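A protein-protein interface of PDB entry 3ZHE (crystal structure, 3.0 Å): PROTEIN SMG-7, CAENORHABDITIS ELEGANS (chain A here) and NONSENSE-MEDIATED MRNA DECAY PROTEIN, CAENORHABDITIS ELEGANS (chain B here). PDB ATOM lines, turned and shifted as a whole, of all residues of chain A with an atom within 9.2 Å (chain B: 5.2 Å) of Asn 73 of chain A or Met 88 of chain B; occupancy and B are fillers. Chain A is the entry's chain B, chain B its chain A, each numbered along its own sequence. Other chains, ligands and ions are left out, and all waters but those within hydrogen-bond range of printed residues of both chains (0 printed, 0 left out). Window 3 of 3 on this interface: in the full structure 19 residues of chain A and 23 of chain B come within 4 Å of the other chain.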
ATOM      1  N   MET A  56      17.938 -26.445  -3.265  1.00  0.00           N
ATOM      2  CA  MET A  56      17.487 -25.442  -4.227  1.00  0.00           C
ATOM      3  C   MET A  56      18.041 -24.059  -3.919  1.00  0.00           C
ATOM      4  O   MET A  56      18.684 -23.436  -4.770  1.00  0.00           O
ATOM      5  CB  MET A  56      15.963 -25.370  -4.248  1.00  0.00           C
ATOM      6  CG  MET A  56      15.309 -26.318  -5.224  1.00  0.00           C
ATOM      7  SD  MET A  56      13.513 -26.191  -5.195  1.00  0.00           S
ATOM      8  CE  MET A  56      13.308 -24.418  -5.332  1.00  0.00           C
ATOM      9  N   MET A  57      17.792 -23.595  -2.698  1.00  0.00           N
ATOM     10  CA  MET A  57      18.274 -22.291  -2.252  1.00  0.00           C
ATOM     11  C   MET A  57      19.776 -22.126  -2.471  1.00  0.00           C
ATOM     12  O   MET A  57      20.226 -21.105  -2.994  1.00  0.00           O
ATOM     13  CB  MET A  57      17.929 -22.073  -0.779  1.00  0.00           C
ATOM     14  CG  MET A  57      16.439 -22.102  -0.489  1.00  0.00           C
ATOM     15  SD  MET A  57      16.063 -21.622   1.206  1.00  0.00           S
ATOM     16  CE  MET A  57      16.789 -19.986   1.264  1.00  0.00           C
ATOM     17  N   ILE A  60      20.858 -22.309  -6.393  1.00  0.00           N
ATOM     18  CA  ILE A  60      20.401 -21.098  -7.068  1.00  0.00           C
ATOM     19  C   ILE A  60      21.154 -19.861  -6.573  1.00  0.00           C
ATOM     20  O   ILE A  60      21.435 -18.947  -7.350  1.00  0.00           O
ATOM     21  CB  ILE A  60      18.873 -20.912  -6.925  1.00  0.00           C
ATOM     22  CG1 ILE A  60      18.138 -22.071  -7.601  1.00  0.00           C
ATOM     23  CG2 ILE A  60      18.424 -19.605  -7.545  1.00  0.00           C
ATOM     24  CD1 ILE A  60      16.626 -21.949  -7.566  1.00  0.00           C
ATOM     25  N   THR A  61      21.496 -19.838  -5.287  1.00  0.00           N
ATOM     26  CA  THR A  61      22.287 -18.739  -4.734  1.00  0.00           C
ATOM     27  C   THR A  61      23.676 -18.705  -5.363  1.00  0.00           C
ATOM     28  O   THR A  61      24.194 -17.639  -5.703  1.00  0.00           O
ATOM     29  CB  THR A  61      22.433 -18.849  -3.203  1.00  0.00           C
ATOM     30  OG1 THR A  61      21.144 -18.729  -2.589  1.00  0.00           O
ATOM     31  CG2 THR A  61      23.346 -17.753  -2.669  1.00  0.00           C
ATOM     32  N   ASP A  67      23.350 -13.029  -6.292  1.00  0.00           N
ATOM     33  CA  ASP A  67      22.494 -11.886  -6.580  1.00  0.00           C
ATOM     34  C   ASP A  67      21.378 -11.800  -5.545  1.00  0.00           C
ATOM     35  O   ASP A  67      20.810 -12.816  -5.147  1.00  0.00           O
ATOM     36  CB  ASP A  67      21.902 -12.008  -7.986  1.00  0.00           C
ATOM     37  CG  ASP A  67      21.072 -10.802  -8.373  1.00  0.00           C
ATOM     38  OD1 ASP A  67      19.871 -10.779  -8.038  1.00  0.00           O
ATOM     39  OD2 ASP A  67      21.620  -9.880  -9.014  1.00  0.00           O
ATOM     40  N   ARG A  68      21.063 -10.582  -5.118  1.00  0.00           N
ATOM     41  CA  ARG A  68      20.064 -10.361  -4.076  1.00  0.00           C
ATOM     42  C   ARG A  68      18.637 -10.646  -4.544  1.00  0.00           C
ATOM     43  O   ARG A  68      17.838 -11.240  -3.810  1.00  0.00           O
ATOM     44  CB  ARG A  68      20.160  -8.929  -3.544  1.00  0.00           C
ATOM     45  N   LEU A  69      18.322 -10.215  -5.761  1.00  0.00           N
ATOM     46  CA  LEU A  69      16.971 -10.353  -6.296  1.00  0.00           C
ATOM     47  C   LEU A  69      16.575 -11.818  -6.437  1.00  0.00           C
ATOM     48  O   LEU A  69      15.452 -12.200  -6.113  1.00  0.00           O
ATOM     49  CB  LEU A  69      16.847  -9.636  -7.643  1.00  0.00           C
ATOM     50  N   VAL A  70      17.508 -12.634  -6.915  1.00  0.00           N
ATOM     51  CA  VAL A  70      17.270 -14.063  -7.064  1.00  0.00           C
ATOM     52  C   VAL A  70      17.117 -14.704  -5.685  1.00  0.00           C
ATOM     53  O   VAL A  70      16.233 -15.542  -5.465  1.00  0.00           O
ATOM     54  CB  VAL A  70      18.427 -14.735  -7.822  1.00  0.00           C
ATOM     55  CG1 VAL A  70      18.032 -16.127  -8.264  1.00  0.00           C
ATOM     56  CG2 VAL A  70      18.829 -13.892  -9.024  1.00  0.00           C
ATOM     57  N   ASN A  71      17.984 -14.287  -4.764  1.00  0.00           N
ATOM     58  CA  ASN A  71      17.956 -14.739  -3.376  1.00  0.00           C
ATOM     59  C   ASN A  71      16.581 -14.582  -2.741  1.00  0.00           C
ATOM     60  O   ASN A  71      15.994 -15.555  -2.263  1.00  0.00           O
ATOM     61  CB  ASN A  71      18.984 -13.964  -2.545  1.00  0.00           C
ATOM     62  CG  ASN A  71      20.086 -14.851  -2.006  1.00  0.00           C
ATOM     63  OD1 ASN A  71      20.476 -15.826  -2.642  1.00  0.00           O
ATOM     64  ND2 ASN A  71      20.588 -14.519  -0.821  1.00  0.00           N
ATOM     65  N   HIS A  72      16.079 -13.348  -2.742  1.00  0.00           N
ATOM     66  CA  HIS A  72      14.757 -13.050  -2.192  1.00  0.00           C
ATOM     67  C   HIS A  72      13.676 -13.932  -2.808  1.00  0.00           C
ATOM     68  O   HIS A  72      12.820 -14.469  -2.100  1.00  0.00           O
ATOM     69  CB  HIS A  72      14.406 -11.575  -2.405  1.00  0.00           C
ATOM     70  CG  HIS A  72      15.062 -10.647  -1.430  1.00  0.00           C
ATOM     71  ND1 HIS A  72      15.655 -11.087  -0.267  1.00  0.00           N
ATOM     72  CD2 HIS A  72      15.215  -9.301  -1.446  1.00  0.00           C
ATOM     73  CE1 HIS A  72      16.147 -10.054   0.393  1.00  0.00           C
ATOM     74  NE2 HIS A  72      15.894  -8.958  -0.302  1.00  0.00           N
ATOM     75  N   ASN A  73      13.733 -14.084  -4.128  1.00  0.00           N
ATOM     76  CA  ASN A  73      12.759 -14.879  -4.863  1.00  0.00           C
ATOM     77  C   ASN A  73      12.723 -16.326  -4.376  1.00  0.00           C
ATOM     78  O   ASN A  73      11.670 -16.828  -3.952  1.00  0.00           O
ATOM     79  CB  ASN A  73      13.059 -14.821  -6.365  1.00  0.00           C
ATOM     80  CG  ASN A  73      11.894 -15.294  -7.213  1.00  0.00           C
ATOM     81  OD1 ASN A  73      11.743 -16.488  -7.468  1.00  0.00           O
ATOM     82  ND2 ASN A  73      11.067 -14.356  -7.660  1.00  0.00           N
ATOM     83  N   VAL A  74      13.877 -16.988  -4.414  1.00  0.00           N
ATOM     84  CA  VAL A  74      13.950 -18.385  -3.991  1.00  0.00           C
ATOM     85  C   VAL A  74      13.616 -18.547  -2.500  1.00  0.00           C
ATOM     86  O   VAL A  74      13.052 -19.566  -2.087  1.00  0.00           O
ATOM     87  CB  VAL A  74      15.317 -19.034  -4.345  1.00  0.00           C
ATOM     88  CG1 VAL A  74      16.402 -18.602  -3.367  1.00  0.00           C
ATOM     89  CG2 VAL A  74      15.196 -20.550  -4.382  1.00  0.00           C
ATOM     90  N   GLN A  75      13.936 -17.527  -1.705  1.00  0.00           N
ATOM     91  CA  GLN A  75      13.624 -17.532  -0.276  1.00  0.00           C
ATOM     92  C   GLN A  75      12.120 -17.531  -0.034  1.00  0.00           C
ATOM     93  O   GLN A  75      11.601 -18.354   0.723  1.00  0.00           O
ATOM     94  CB  GLN A  75      14.259 -16.328   0.427  1.00  0.00           C
ATOM     95  CG  GLN A  75      15.753 -16.457   0.693  1.00  0.00           C
ATOM     96  CD  GLN A  75      16.353 -15.178   1.248  1.00  0.00           C
ATOM     97  OE1 GLN A  75      15.742 -14.110   1.177  1.00  0.00           O
ATOM     98  NE2 GLN A  75      17.552 -15.281   1.808  1.00  0.00           N
ATOM     99  N   ASN A  76      11.421 -16.599  -0.674  1.00  0.00           N
ATOM    100  CA  ASN A  76       9.970 -16.530  -0.556  1.00  0.00           C
ATOM    101  C   ASN A  76       9.299 -17.793  -1.095  1.00  0.00           C
ATOM    102  O   ASN A  76       8.294 -18.256  -0.540  1.00  0.00           O
ATOM    103  CB  ASN A  76       9.425 -15.277  -1.247  1.00  0.00           C
ATOM    104  CG  ASN A  76       9.866 -13.996  -0.563  1.00  0.00           C
ATOM    105  OD1 ASN A  76      10.094 -13.970   0.646  1.00  0.00           O
ATOM    106  ND2 ASN A  76       9.989 -12.924  -1.338  1.00  0.00           N
ATOM    107  N   LEU A  77       9.863 -18.354  -2.164  1.00  0.00           N
ATOM    108  CA  LEU A  77       9.384 -19.638  -2.671  1.00  0.00           C
ATOM    109  C   LEU A  77       9.484 -20.706  -1.583  1.00  0.00           C
ATOM    110  O   LEU A  77       8.538 -21.466  -1.346  1.00  0.00           O
ATOM    111  CB  LEU A  77      10.185 -20.069  -3.900  1.00  0.00           C
ATOM    112  CG  LEU A  77       9.877 -21.466  -4.447  1.00  0.00           C
ATOM    113  CD1 LEU A  77       8.413 -21.581  -4.835  1.00  0.00           C
ATOM    114  CD2 LEU A  77      10.771 -21.788  -5.633  1.00  0.00           C
ATOM    115  N   ALA A  78      10.636 -20.741  -0.919  1.00  0.00           N
ATOM    116  CA  ALA A  78      10.866 -21.656   0.194  1.00  0.00           C
ATOM    117  C   ALA A  78       9.817 -21.495   1.295  1.00  0.00           C
ATOM    118  O   ALA A  78       9.205 -22.478   1.735  1.00  0.00           O
ATOM    119  CB  ALA A  78      12.261 -21.449   0.758  1.00  0.00           C
ATOM    120  N   ILE A  79       9.621 -20.252   1.735  1.00  0.00           N
ATOM    121  CA  ILE A  79       8.627 -19.933   2.758  1.00  0.00           C
ATOM    122  C   ILE A  79       7.256 -20.474   2.369  1.00  0.00           C
ATOM    123  O   ILE A  79       6.567 -21.104   3.183  1.00  0.00           O
ATOM    124  CB  ILE A  79       8.523 -18.410   2.989  1.00  0.00           C
ATOM    125  CG1 ILE A  79       9.816 -17.868   3.603  1.00  0.00           C
ATOM    126  CG2 ILE A  79       7.334 -18.082   3.879  1.00  0.00           C
ATOM    127  CD1 ILE A  79       9.805 -16.367   3.817  1.00  0.00           C
ATOM    128  N   GLY A  80       6.874 -20.236   1.116  1.00  0.00           N
ATOM    129  CA  GLY A  80       5.623 -20.749   0.590  1.00  0.00           C
ATOM    130  C   GLY A  80       5.520 -22.258   0.705  1.00  0.00           C
ATOM    131  O   GLY A  80       4.543 -22.782   1.250  1.00  0.00           O
ATOM    132  N   PHE A  81       6.534 -22.958   0.202  1.00  0.00           N
ATOM    133  CA  PHE A  81       6.542 -24.419   0.248  1.00  0.00           C
ATOM    134  C   PHE A  81       6.406 -24.973   1.669  1.00  0.00           C
ATOM    135  O   PHE A  81       5.586 -25.858   1.921  1.00  0.00           O
ATOM    136  CB  PHE A  81       7.800 -24.981  -0.424  1.00  0.00           C
ATOM    137  CG  PHE A  81       7.590 -25.405  -1.851  1.00  0.00           C
ATOM    138  CD1 PHE A  81       6.886 -26.560  -2.149  1.00  0.00           C
ATOM    139  CD2 PHE A  81       8.110 -24.657  -2.894  1.00  0.00           C
ATOM    140  CE1 PHE A  81       6.696 -26.953  -3.461  1.00  0.00           C
ATOM    141  CE2 PHE A  81       7.924 -25.047  -4.208  1.00  0.00           C
ATOM    142  CZ  PHE A  81       7.216 -26.196  -4.491  1.00  0.00           C
ATOM    143  N   ASP A  84       2.958 -24.178   3.293  1.00  0.00           N
ATOM    144  CA  ASP A  84       1.969 -25.054   2.680  1.00  0.00           C
ATOM    145  C   ASP A  84       2.117 -26.500   3.141  1.00  0.00           C
ATOM    146  O   ASP A  84       1.131 -27.226   3.225  1.00  0.00           O
ATOM    147  CB  ASP A  84       2.018 -24.958   1.154  1.00  0.00           C
ATOM    148  CG  ASP A  84       1.366 -23.694   0.636  1.00  0.00           C
ATOM    149  OD1 ASP A  84       0.651 -23.036   1.421  1.00  0.00           O
ATOM    150  OD2 ASP A  84       1.557 -23.365  -0.554  1.00  0.00           O
ATOM    151  N   LYS A 143      16.155 -14.254   5.657  1.00  0.00           N
ATOM    152  CA  LYS A 143      15.486 -13.046   5.186  1.00  0.00           C
ATOM    153  C   LYS A 143      15.801 -11.848   6.084  1.00  0.00           C
ATOM    154  O   LYS A 143      15.230 -10.767   5.924  1.00  0.00           O
ATOM    155  CB  LYS A 143      13.976 -13.280   5.120  1.00  0.00           C
ATOM    156  CG  LYS A 143      13.232 -12.347   4.185  1.00  0.00           C
ATOM    157  CD  LYS A 143      11.757 -12.689   4.145  1.00  0.00           C
ATOM    158  CE  LYS A 143      10.993 -11.711   3.275  1.00  0.00           C
ATOM    159  NZ  LYS A 143       9.555 -12.076   3.197  1.00  0.00           N
ATOM    160  N   ARG B  36       7.138  -4.739  -6.541  1.00  0.00           N
ATOM    161  CA  ARG B  36       6.260  -5.396  -5.579  1.00  0.00           C
ATOM    162  C   ARG B  36       6.812  -5.248  -4.167  1.00  0.00           C
ATOM    163  O   ARG B  36       6.071  -4.931  -3.232  1.00  0.00           O
ATOM    164  CB  ARG B  36       6.068  -6.879  -5.919  1.00  0.00           C
ATOM    165  CG  ARG B  36       5.232  -7.142  -7.161  1.00  0.00           C
ATOM    166  CD  ARG B  36       4.603  -8.530  -7.132  1.00  0.00           C
ATOM    167  NE  ARG B  36       5.578  -9.595  -6.910  1.00  0.00           N
ATOM    168  CZ  ARG B  36       6.222 -10.238  -7.879  1.00  0.00           C
ATOM    169  NH1 ARG B  36       6.003  -9.923  -9.149  1.00  0.00           N
ATOM    170  NH2 ARG B  36       7.089 -11.196  -7.578  1.00  0.00           N
ATOM    171  N   ALA B  83       1.852 -23.808 -10.628  1.00  0.00           N
ATOM    172  CA  ALA B  83       1.721 -24.060  -9.199  1.00  0.00           C
ATOM    173  C   ALA B  83       2.926 -23.522  -8.429  1.00  0.00           C
ATOM    174  O   ALA B  83       2.782 -23.003  -7.322  1.00  0.00           O
ATOM    175  CB  ALA B  83       1.534 -25.549  -8.935  1.00  0.00           C
ATOM    176  N   VAL B  84       4.109 -23.641  -9.025  1.00  0.00           N
ATOM    177  CA  VAL B  84       5.339 -23.160  -8.403  1.00  0.00           C
ATOM    178  C   VAL B  84       5.336 -21.640  -8.262  1.00  0.00           C
ATOM    179  O   VAL B  84       5.619 -21.108  -7.185  1.00  0.00           O
ATOM    180  CB  VAL B  84       6.583 -23.587  -9.202  1.00  0.00           C
ATOM    181  CG1 VAL B  84       7.844 -23.031  -8.560  1.00  0.00           C
ATOM    182  CG2 VAL B  84       6.653 -25.102  -9.301  1.00  0.00           C
ATOM    183  N   LEU B  85       5.018 -20.952  -9.357  1.00  0.00           N
ATOM    184  CA  LEU B  85       4.904 -19.496  -9.356  1.00  0.00           C
ATOM    185  C   LEU B  85       3.901 -19.040  -8.308  1.00  0.00           C
ATOM    186  O   LEU B  85       4.155 -18.097  -7.549  1.00  0.00           O
ATOM    187  CB  LEU B  85       4.473 -18.991 -10.733  1.00  0.00           C
ATOM    188  CG  LEU B  85       4.096 -17.509 -10.804  1.00  0.00           C
ATOM    189  CD1 LEU B  85       5.280 -16.627 -10.446  1.00  0.00           C
ATOM    190  CD2 LEU B  85       3.560 -17.150 -12.177  1.00  0.00           C
ATOM    191  N   LEU B  86       2.759 -19.719  -8.273  1.00  0.00           N
ATOM    192  CA  LEU B  86       1.728 -19.412  -7.291  1.00  0.00           C
ATOM    193  C   LEU B  86       2.240 -19.592  -5.868  1.00  0.00           C
ATOM    194  O   LEU B  86       1.936 -18.788  -4.986  1.00  0.00           O
ATOM    195  CB  LEU B  86       0.487 -20.270  -7.529  1.00  0.00           C
ATOM    196  CG  LEU B  86      -0.377 -19.794  -8.695  1.00  0.00           C
ATOM    197  CD1 LEU B  86      -1.430 -20.827  -9.052  1.00  0.00           C
ATOM    198  CD2 LEU B  86      -1.029 -18.466  -8.350  1.00  0.00           C
ATOM    199  N   THR B  87       3.026 -20.642  -5.651  1.00  0.00           N
ATOM    200  CA  THR B  87       3.624 -20.893  -4.344  1.00  0.00           C
ATOM    201  C   THR B  87       4.572 -19.764  -3.942  1.00  0.00           C
ATOM    202  O   THR B  87       4.550 -19.298  -2.800  1.00  0.00           O
ATOM    203  CB  THR B  87       4.373 -22.239  -4.311  1.00  0.00           C
ATOM    204  OG1 THR B  87       3.460 -23.302  -4.607  1.00  0.00           O
ATOM    205  CG2 THR B  87       4.985 -22.475  -2.941  1.00  0.00           C
ATOM    206  N   MET B  88       5.397 -19.325  -4.889  1.00  0.00           N
ATOM    207  CA  MET B  88       6.308 -18.212  -4.648  1.00  0.00           C
ATOM    208  C   MET B  88       5.523 -16.970  -4.249  1.00  0.00           C
ATOM    209  O   MET B  88       5.891 -16.268  -3.307  1.00  0.00           O
ATOM    210  CB  MET B  88       7.130 -17.911  -5.899  1.00  0.00           C
ATOM    211  CG  MET B  88       8.134 -16.786  -5.719  1.00  0.00           C
ATOM    212  SD  MET B  88       8.550 -15.968  -7.273  1.00  0.00           S
ATOM    213  CE  MET B  88       7.016 -15.121  -7.631  1.00  0.00           C
ATOM    214  N   PHE B  89       4.441 -16.708  -4.979  1.00  0.00           N
ATOM    215  CA  PHE B  89       3.550 -15.597  -4.662  1.00  0.00           C
ATOM    216  C   PHE B  89       2.982 -15.717  -3.246  1.00  0.00           C
ATOM    217  O   PHE B  89       2.865 -14.722  -2.526  1.00  0.00           O
ATOM    218  CB  PHE B  89       2.413 -15.516  -5.684  1.00  0.00           C
ATOM    219  CG  PHE B  89       2.749 -14.704  -6.902  1.00  0.00           C
ATOM    220  CD1 PHE B  89       3.741 -13.740  -6.853  1.00  0.00           C
ATOM    221  CD2 PHE B  89       2.068 -14.900  -8.092  1.00  0.00           C
ATOM    222  CE1 PHE B  89       4.050 -12.990  -7.968  1.00  0.00           C
ATOM    223  CE2 PHE B  89       2.374 -14.151  -9.210  1.00  0.00           C
ATOM    224  CZ  PHE B  89       3.367 -13.195  -9.146  1.00  0.00           C
ATOM    225  N   CYS B  90       2.638 -16.941  -2.852  1.00  0.00           N
ATOM    226  CA  CYS B  90       2.099 -17.193  -1.519  1.00  0.00           C
ATOM    227  C   CYS B  90       3.123 -16.884  -0.437  1.00  0.00           C
ATOM    228  O   CYS B  90       2.813 -16.215   0.549  1.00  0.00           O
ATOM    229  CB  CYS B  90       1.634 -18.643  -1.385  1.00  0.00           C
ATOM    230  SG  CYS B  90       0.219 -19.073  -2.413  1.00  0.00           S
ATOM    231  N   GLY B  91       4.343 -17.380  -0.622  1.00  0.00           N
ATOM    232  CA  GLY B  91       5.417 -17.112   0.313  1.00  0.00           C
ATOM    233  C   GLY B  91       5.739 -15.634   0.372  1.00  0.00           C
ATOM    234  O   GLY B  91       6.181 -15.119   1.403  1.00  0.00           O
ATOM    235  N   GLU B  92       5.511 -14.948  -0.742  1.00  0.00           N
ATOM    236  CA  GLU B  92       5.763 -13.520  -0.825  1.00  0.00           C
ATOM    237  C   GLU B  92       4.715 -12.751  -0.028  1.00  0.00           C
ATOM    238  O   GLU B  92       5.042 -11.803   0.683  1.00  0.00           O
ATOM    239  CB  GLU B  92       5.763 -13.070  -2.286  1.00  0.00           C
ATOM    240  CG  GLU B  92       6.504 -11.775  -2.540  1.00  0.00           C
ATOM    241  CD  GLU B  92       6.776 -11.541  -4.012  1.00  0.00           C
ATOM    242  OE1 GLU B  92       6.388 -12.395  -4.839  1.00  0.00           O
ATOM    243  OE2 GLU B  92       7.381 -10.502  -4.342  1.00  0.00           O
ATOM    244  N   LEU B  93       3.459 -13.169  -0.141  1.00  0.00           N
ATOM    245  CA  LEU B  93       2.364 -12.498   0.556  1.00  0.00           C
ATOM    246  C   LEU B  93       2.233 -12.944   2.010  1.00  0.00           C
ATOM    247  O   LEU B  93       1.461 -12.366   2.774  1.00  0.00           O
ATOM    248  CB  LEU B  93       1.038 -12.720  -0.172  1.00  0.00           C
ATOM    249  CG  LEU B  93       0.696 -11.740  -1.296  1.00  0.00           C
ATOM    250  CD1 LEU B  93      -0.706 -12.000  -1.822  1.00  0.00           C
ATOM    251  CD2 LEU B  93       0.830 -10.303  -0.815  1.00  0.00           C
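OE1 of Glu 92 of chain B is in salt-bridge range of NH2 of Arg 36 of chain B. The side-chain hydroxyl of Thr 87 of chain B is in hydrogen-bond range of the backbone carbonyl oxygen of Ala 83 of chain B (2.8 Å). O of His 72 of chain A is in hydrogen-bond range of ND2 of Asn 76 of chain A (3.3 Å). The side-chain amino group of Lys 143 of chain A lies within hydrogen-bond range of the side-chain amide oxygen of Asn 76 of chain A, 3.2 Å away.
SD of Met 88 of chain B sits at hydrogen-bond distance from ND2 of Asn 73 of chain A.
Printed residues of chain B that touch a printed residue of chain A: Val 84, Thr 87, Met 88, Gly 91 and Glu 92. Hydrophobic or aromatic side chains of chain B within 4 Å of the printed part of chain A: Met 88. Of the 21 printed residues of chain A, 5 touch a printed residue of chain B. Among the printed residues, 8 pairs touch across the chains. Among the printed residues, no Asp or Glu carboxylate lies within 4 Å of a Lys or Arg side-chain nitrogen of the other chain.
O of Asn 76 of chain A touches CA of Gly 91 of chain B (3.2 Å). Asn 76 of chain A touches Glu 92 of chain B (ND2 to CG, 3.9 Å). O of Val 84 of chain B touches CD1 of Leu 77 of chain A, 3.7 Å away. CD1 of Leu 77 of chain A touches N of Met 88 of chain B, at 3.8 Å. Thr 87 of chain B touches Gly 80 of chain A (CG2 to C, 3.7 Å). Gly 80 of chain A touches Gly 91 of chain B (N to CA, 3.5 Å). Thr 87 of chain B touches Phe 81 of chain A.
Of chain B, only Met 88 (3.0 Å) comes within 4 Å of Asn 73 of chain A. Met 88 of chain B touches just these residues of chain A: Asn 73 and Leu 77. No residue of chain A comes within 4 Å of Phe 89 of chain B. Of chain A, only Asn 76 (3.2 Å) and Gly 80 (3.5 Å) come within 4 Å of Gly 91 of chain B. Of the printed residues of chain A, Val 84 of chain B touches Leu 77. Of the printed residues of chain B, Gly 80 of chain A touches Thr 87 and Gly 91. Leu 69 of chain A touches none of the printed residues of chain B. Ile 79 of chain A touches none of the printed residues of chain B. The nearest printed residue of chain B that does not touch Gly 80 of chain A is Cys 90 of chain B (4.7 Å).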
